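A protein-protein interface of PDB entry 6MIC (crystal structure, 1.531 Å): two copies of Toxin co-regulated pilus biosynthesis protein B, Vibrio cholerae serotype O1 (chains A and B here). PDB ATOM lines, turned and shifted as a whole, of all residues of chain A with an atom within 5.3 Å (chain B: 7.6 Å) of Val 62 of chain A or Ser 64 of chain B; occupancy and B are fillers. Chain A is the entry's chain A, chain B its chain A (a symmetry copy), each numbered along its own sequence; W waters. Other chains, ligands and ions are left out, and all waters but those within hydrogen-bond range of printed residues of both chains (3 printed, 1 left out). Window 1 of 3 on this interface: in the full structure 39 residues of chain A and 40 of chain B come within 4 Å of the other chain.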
ATOM      1  N   LYS A  59      20.665  15.259  22.510  1.00  0.00           N
ATOM      2  CA  LYS A  59      21.428  14.067  22.833  1.00  0.00           C
ATOM      3  C   LYS A  59      21.933  13.424  21.559  1.00  0.00           C
ATOM      4  O   LYS A  59      21.396  13.631  20.469  1.00  0.00           O
ATOM      5  CB  LYS A  59      20.568  13.061  23.602  1.00  0.00           C
ATOM      6  CG  LYS A  59      20.285  13.514  25.072  1.00  0.00           C
ATOM      7  CD  LYS A  59      19.285  12.621  25.790  1.00  0.00           C
ATOM      8  CE  LYS A  59      19.194  12.889  27.287  1.00  0.00           C
ATOM      9  NZ  LYS A  59      20.257  12.230  28.100  1.00  0.00           N
ATOM     10  N   THR A  60      22.987  12.621  21.716  1.00  0.00           N
ATOM     11  CA  THR A  60      23.351  11.670  20.688  1.00  0.00           C
ATOM     12  C   THR A  60      22.989  10.284  21.196  1.00  0.00           C
ATOM     13  O   THR A  60      22.764  10.079  22.394  1.00  0.00           O
ATOM     14  CB  THR A  60      24.844  11.750  20.332  1.00  0.00           C
ATOM     15  OG1 THR A  60      25.610  11.416  21.481  1.00  0.00           O
ATOM     16  CG2 THR A  60      25.201  13.149  19.826  1.00  0.00           C
ATOM     17  N   PRO A  61      22.941   9.289  20.315  1.00  0.00           N
ATOM     18  CA  PRO A  61      22.516   7.951  20.737  1.00  0.00           C
ATOM     19  C   PRO A  61      23.475   7.322  21.734  1.00  0.00           C
ATOM     20  O   PRO A  61      24.699   7.473  21.633  1.00  0.00           O
ATOM     21  CB  PRO A  61      22.506   7.153  19.425  1.00  0.00           C
ATOM     22  CG  PRO A  61      22.401   8.125  18.369  1.00  0.00           C
ATOM     23  CD  PRO A  61      23.143   9.364  18.872  1.00  0.00           C
ATOM     24  N   VAL A  62      22.934   6.565  22.684  1.00  0.00           N
ATOM     25  CA  VAL A  62      23.803   5.878  23.620  1.00  0.00           C
ATOM     26  C   VAL A  62      24.525   4.756  22.888  1.00  0.00           C
ATOM     27  O   VAL A  62      23.942   4.042  22.045  1.00  0.00           O
ATOM     28  CB  VAL A  62      23.067   5.321  24.849  1.00  0.00           C
ATOM     29  CG1 VAL A  62      22.350   6.399  25.620  1.00  0.00           C
ATOM     30  CG2 VAL A  62      22.147   4.198  24.460  1.00  0.00           C
ATOM     31  N   VAL A  63      25.802   4.616  23.174  1.00  0.00           N
ATOM     32  CA  VAL A  63      26.620   3.575  22.588  1.00  0.00           C
ATOM     33  C   VAL A  63      27.273   2.797  23.718  1.00  0.00           C
ATOM     34  O   VAL A  63      27.718   3.382  24.708  1.00  0.00           O
ATOM     35  CB  VAL A  63      27.636   4.155  21.582  1.00  0.00           C
ATOM     36  CG1 VAL A  63      26.883   4.675  20.379  1.00  0.00           C
ATOM     37  CG2 VAL A  63      28.477   5.264  22.172  1.00  0.00           C
ATOM     38  N   SER A  64      27.271   1.468  23.576  1.00  0.00           N
ATOM     39  CA  SER A  64      27.576   0.509  24.627  1.00  0.00           C
ATOM     40  C   SER A  64      28.811  -0.308  24.276  1.00  0.00           C
ATOM     41  O   SER A  64      29.005  -0.707  23.120  1.00  0.00           O
ATOM     42  CB  SER A  64      26.378  -0.439  24.863  1.00  0.00           C
ATOM     43  OG  SER A  64      25.751  -0.871  23.645  1.00  0.00           O
ATOM     44  N   PHE A 180      28.253   2.876  28.926  1.00  0.00           N
ATOM     45  CA  PHE A 180      27.411   3.632  28.026  1.00  0.00           C
ATOM     46  C   PHE A 180      27.990   5.027  27.881  1.00  0.00           C
ATOM     47  O   PHE A 180      28.312   5.658  28.890  1.00  0.00           O
ATOM     48  CB  PHE A 180      25.976   3.734  28.561  1.00  0.00           C
ATOM     49  CG  PHE A 180      25.215   2.427  28.543  1.00  0.00           C
ATOM     50  CD1 PHE A 180      24.458   2.095  27.443  1.00  0.00           C
ATOM     51  CD2 PHE A 180      25.275   1.548  29.607  1.00  0.00           C
ATOM     52  CE1 PHE A 180      23.753   0.905  27.406  1.00  0.00           C
ATOM     53  CE2 PHE A 180      24.551   0.367  29.574  1.00  0.00           C
ATOM     54  CZ  PHE A 180      23.799   0.060  28.461  1.00  0.00           C
ATOM     55  N   GLN A 181      28.127   5.492  26.654  1.00  0.00           N
ATOM     56  CA  GLN A 181      28.557   6.860  26.389  1.00  0.00           C
ATOM     57  C   GLN A 181      27.522   7.522  25.504  1.00  0.00           C
ATOM     58  O   GLN A 181      26.902   6.868  24.667  1.00  0.00           O
ATOM     59  CB  GLN A 181      29.940   6.914  25.704  1.00  0.00           C
ATOM     60  CG  GLN A 181      31.092   6.510  26.618  1.00  0.00           C
ATOM     61  CD  GLN A 181      32.414   6.895  26.062  1.00  0.00           C
ATOM     62  OE1 GLN A 181      32.656   8.053  25.744  1.00  0.00           O
ATOM     63  NE2 GLN A 181      33.298   5.920  25.948  1.00  0.00           N
ATOM     64  N   TRP A 182      27.363   8.830  25.674  1.00  0.00           N
ATOM     65  CA  TRP A 182      26.543   9.651  24.796  1.00  0.00           C
ATOM     66  C   TRP A 182      26.968  11.087  25.015  1.00  0.00           C
ATOM     67  O   TRP A 182      27.745  11.388  25.919  1.00  0.00           O
ATOM     68  CB  TRP A 182      25.041   9.484  25.067  1.00  0.00           C
ATOM     69  CG  TRP A 182      24.553  10.042  26.399  1.00  0.00           C
ATOM     70  CD1 TRP A 182      23.890  11.234  26.603  1.00  0.00           C
ATOM     71  CD2 TRP A 182      24.692   9.439  27.684  1.00  0.00           C
ATOM     72  NE1 TRP A 182      23.602  11.384  27.930  1.00  0.00           N
ATOM     73  CE2 TRP A 182      24.094  10.314  28.622  1.00  0.00           C
ATOM     74  CE3 TRP A 182      25.282   8.257  28.151  1.00  0.00           C
ATOM     75  CZ2 TRP A 182      24.042  10.027  29.980  1.00  0.00           C
ATOM     76  CZ3 TRP A 182      25.228   7.974  29.500  1.00  0.00           C
ATOM     77  CH2 TRP A 182      24.623   8.863  30.407  1.00  0.00           C
ATOM     78  N   GLU A 184      25.493  15.224  25.316  1.00  0.00           N
ATOM     79  CA  GLU A 184      24.316  15.951  25.783  1.00  0.00           C
ATOM     80  C   GLU A 184      24.679  17.414  26.027  1.00  0.00           C
ATOM     81  O   GLU A 184      25.800  17.721  26.442  1.00  0.00           O
ATOM     82  CB  GLU A 184      23.784  15.316  27.074  1.00  0.00           C
ATOM     83  CG  GLU A 184      22.509  15.879  27.623  1.00  0.00           C
ATOM     84  CD  GLU A 184      22.024  15.085  28.823  1.00  0.00           C
ATOM     85  OE1 GLU A 184      21.429  15.695  29.736  1.00  0.00           O
ATOM     86  OE2 GLU A 184      22.255  13.853  28.859  1.00  0.00           O
ATOM     87  N   PRO B  61      14.646   6.675  20.845  1.00  0.00           N
ATOM     88  CA  PRO B  61      15.958   6.316  21.393  1.00  0.00           C
ATOM     89  C   PRO B  61      15.951   6.221  22.910  1.00  0.00           C
ATOM     90  O   PRO B  61      15.295   7.010  23.602  1.00  0.00           O
ATOM     91  CB  PRO B  61      16.860   7.470  20.932  1.00  0.00           C
ATOM     92  CG  PRO B  61      16.198   8.067  19.803  1.00  0.00           C
ATOM     93  CD  PRO B  61      14.700   7.911  20.072  1.00  0.00           C
ATOM     94  N   VAL B  62      16.722   5.282  23.450  1.00  0.00           N
ATOM     95  CA  VAL B  62      16.814   5.189  24.894  1.00  0.00           C
ATOM     96  C   VAL B  62      17.600   6.385  25.415  1.00  0.00           C
ATOM     97  O   VAL B  62      18.611   6.814  24.819  1.00  0.00           O
ATOM     98  CB  VAL B  62      17.452   3.882  25.389  1.00  0.00           C
ATOM     99  CG1 VAL B  62      16.699   2.665  24.914  1.00  0.00           C
ATOM    100  CG2 VAL B  62      18.908   3.822  25.019  1.00  0.00           C
ATOM    101  N   VAL B  63      17.122   6.952  26.501  1.00  0.00           N
ATOM    102  CA  VAL B  63      17.772   8.078  27.139  1.00  0.00           C
ATOM    103  C   VAL B  63      18.013   7.721  28.596  1.00  0.00           C
ATOM    104  O   VAL B  63      17.156   7.115  29.244  1.00  0.00           O
ATOM    105  CB  VAL B  63      16.959   9.377  26.958  1.00  0.00           C
ATOM    106  CG1 VAL B  63      17.002   9.776  25.501  1.00  0.00           C
ATOM    107  CG2 VAL B  63      15.521   9.233  27.402  1.00  0.00           C
ATOM    108  N   SER B  64      19.213   8.055  29.080  1.00  0.00           N
ATOM    109  CA  SER B  64      19.778   7.580  30.333  1.00  0.00           C
ATOM    110  C   SER B  64      20.012   8.734  31.296  1.00  0.00           C
ATOM    111  O   SER B  64      20.449   9.822  30.895  1.00  0.00           O
ATOM    112  CB  SER B  64      21.109   6.836  30.083  1.00  0.00           C
ATOM    113  OG  SER B  64      21.944   7.483  29.109  1.00  0.00           O
ATOM    114  N   THR B  65      19.743   8.465  32.577  1.00  0.00           N
ATOM    115  CA  THR B  65      19.979   9.395  33.669  1.00  0.00           C
ATOM    116  C   THR B  65      20.529   8.612  34.853  1.00  0.00           C
ATOM    117  O   THR B  65      20.015   7.541  35.184  1.00  0.00           O
ATOM    118  CB  THR B  65      18.691  10.099  34.084  1.00  0.00           C
ATOM    119  OG1 THR B  65      18.119  10.734  32.927  1.00  0.00           O
ATOM    120  CG2 THR B  65      18.937  11.129  35.156  1.00  0.00           C
ATOM    121  N   TYR B  66      21.529   9.178  35.524  1.00  0.00           N
ATOM    122  CA  TYR B  66      22.044   8.667  36.794  1.00  0.00           C
ATOM    123  C   TYR B  66      21.150   9.084  37.963  1.00  0.00           C
ATOM    124  O   TYR B  66      20.844  10.272  38.130  1.00  0.00           O
ATOM    125  CB  TYR B  66      23.447   9.216  36.976  1.00  0.00           C
ATOM    126  CG  TYR B  66      24.230   8.709  38.154  1.00  0.00           C
ATOM    127  CD1 TYR B  66      25.107   7.639  38.025  1.00  0.00           C
ATOM    128  CD2 TYR B  66      24.148   9.345  39.389  1.00  0.00           C
ATOM    129  CE1 TYR B  66      25.828   7.204  39.093  1.00  0.00           C
ATOM    130  CE2 TYR B  66      24.871   8.898  40.477  1.00  0.00           C
ATOM    131  CZ  TYR B  66      25.734   7.840  40.309  1.00  0.00           C
ATOM    132  OH  TYR B  66      26.498   7.344  41.335  1.00  0.00           O
ATOM    133  N   GLU B  67      20.784   8.128  38.821  1.00  0.00           N
ATOM    134  CA  GLU B  67      19.767   8.354  39.840  1.00  0.00           C
ATOM    135  C   GLU B  67      20.181   7.791  41.191  1.00  0.00           C
ATOM    136  O   GLU B  67      20.812   6.734  41.280  1.00  0.00           O
ATOM    137  CB  GLU B  67      18.418   7.713  39.437  1.00  0.00           C
ATOM    138  CG  GLU B  67      17.840   8.268  38.130  1.00  0.00           C
ATOM    139  CD  GLU B  67      17.309   9.678  38.230  1.00  0.00           C
ATOM    140  OE1 GLU B  67      16.879  10.190  37.167  1.00  0.00           O
ATOM    141  OE2 GLU B  67      17.328  10.283  39.318  1.00  0.00           O
ATOM    142  N   ILE B 178      21.042   3.500  36.955  1.00  0.00           N
ATOM    143  CA  ILE B 178      20.827   4.209  35.707  1.00  0.00           C
ATOM    144  C   ILE B 178      19.386   3.961  35.308  1.00  0.00           C
ATOM    145  O   ILE B 178      18.939   2.804  35.224  1.00  0.00           O
ATOM    146  CB  ILE B 178      21.804   3.766  34.615  1.00  0.00           C
ATOM    147  CG1 ILE B 178      23.255   3.796  35.123  1.00  0.00           C
ATOM    148  CG2 ILE B 178      21.615   4.667  33.379  1.00  0.00           C
ATOM    149  CD1 ILE B 178      23.688   5.132  35.703  1.00  0.00           C
ATOM    150  N   ALA B 179      18.642   5.043  35.107  1.00  0.00           N
ATOM    151  CA  ALA B 179      17.284   4.998  34.609  1.00  0.00           C
ATOM    152  C   ALA B 179      17.303   5.190  33.100  1.00  0.00           C
ATOM    153  O   ALA B 179      17.878   6.172  32.595  1.00  0.00           O
ATOM    154  CB  ALA B 179      16.449   6.077  35.296  1.00  0.00           C
ATOM    155  N   PHE B 180      16.759   4.228  32.380  1.00  0.00           N
ATOM    156  CA  PHE B 180      16.587   4.297  30.947  1.00  0.00           C
ATOM    157  C   PHE B 180      15.117   4.522  30.647  1.00  0.00           C
ATOM    158  O   PHE B 180      14.269   3.822  31.203  1.00  0.00           O
ATOM    159  CB  PHE B 180      17.047   3.000  30.269  1.00  0.00           C
ATOM    160  CG  PHE B 180      18.543   2.778  30.311  1.00  0.00           C
ATOM    161  CD1 PHE B 180      19.329   3.238  29.279  1.00  0.00           C
ATOM    162  CD2 PHE B 180      19.143   2.131  31.374  1.00  0.00           C
ATOM    163  CE1 PHE B 180      20.699   3.043  29.296  1.00  0.00           C
ATOM    164  CE2 PHE B 180      20.511   1.921  31.377  1.00  0.00           C
ATOM    165  CZ  PHE B 180      21.275   2.391  30.330  1.00  0.00           C
ATOM    166  N   GLN B 181      14.822   5.484  29.793  1.00  0.00           N
ATOM    167  CA  GLN B 181      13.458   5.718  29.332  1.00  0.00           C
ATOM    168  C   GLN B 181      13.454   5.676  27.819  1.00  0.00           C
ATOM    169  O   GLN B 181      14.426   6.066  27.176  1.00  0.00           O
ATOM    170  CB  GLN B 181      12.904   7.075  29.817  1.00  0.00           C
ATOM    171  CG  GLN B 181      12.625   7.123  31.315  1.00  0.00           C
ATOM    172  CD  GLN B 181      11.784   8.286  31.695  1.00  0.00           C
ATOM    173  OE1 GLN B 181      10.697   8.484  31.167  1.00  0.00           O
ATOM    174  NE2 GLN B 181      12.279   9.071  32.636  1.00  0.00           N
HETATM  175  O   HOH W   1      20.017   6.733  22.762  1.00  0.00           O
HETATM  176  O   HOH W   2      21.251  12.318  31.460  1.00  0.00           O
HETATM  177  O   HOH W   3      20.754   9.309  24.240  1.00  0.00           O
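The backbone NH (N) of Gln 181 of chain B lies within hydrogen-bond range of the backbone carbonyl oxygen (O) of Val 63 of chain B (2.9 Å). NE1 of Trp 182 of chain A is in hydrogen-bond range of OE2 of Glu 184 of chain A (3.0 Å). The side-chain amino group (NZ) of Lys 59 of chain A lies within salt-bridge range of the side-chain carboxylate (OE2) of Glu 184 of chain A.
CG1 of Val 63 of chain B touches CD of Lys 59 of chain A (3.7 Å). Lys 59 of chain A touches Ser 64 of chain B. CG2 of Val 62 of chain A touches CG2 of Val 62 of chain B (3.3 Å). CG1 of Val 62 of chain A touches OG of Ser 64 of chain B (3.7 Å). Phe 180 of chain A touches Phe 180 of chain B (CZ to CZ, 3.9 Å). Trp 182 of chain A touches Ser 64 of chain B (CH2 to OG, 3.3 Å).
Ser 64 of chain A touches none of the printed residues of chain B. Printed residues of chain B within 4 Å of Trp 182 of chain A: Ser 64. Of the printed residues of chain A, Val 62 of chain B touches Val 62. Printed residues of chain A within 4 Å of Phe 180 of chain B: Phe 180. The nearest printed residue of chain A that does not touch Val 62 of chain B is Pro 61 of chain A (5.8 Å).
Hydrophobic or aromatic side chains of chain A that line the printed part of chain B: Val 62, Phe 180 and Trp 182. Among the printed residues, 6 pairs touch across the chains. Among the printed residues, no Asp or Glu carboxylate lies within 4 Å of a Lys or Arg side-chain nitrogen of the other chain.
Val 62 of chain A touches its own counterpart, Val 62 of chain B. Val 62 of chain A touches Ser 64 of chain B, but with the chains exchanged Ser 64 of chain A does not touch Val 62 of chain B (8.4 Å). Phe 180 of chain B touches its own counterpart, Phe 180 of chain A. Of the 6 pairs that touch across the chains among the printed residues, 2 have their exchanged pair printed and touching as well.
Water W1 lies within hydrogen-bond range of O of Val 62 of chain B and N of Val 62 of chain A. Water W2 lies within hydrogen-bond range of O of Ser 64 of chain B and OE2 of Glu 184 of chain A. Water W3 bridges the backbone carbonyl oxygen of Thr 60 of chain A and the backbone carbonyl oxygen of Val 62 of chain B.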
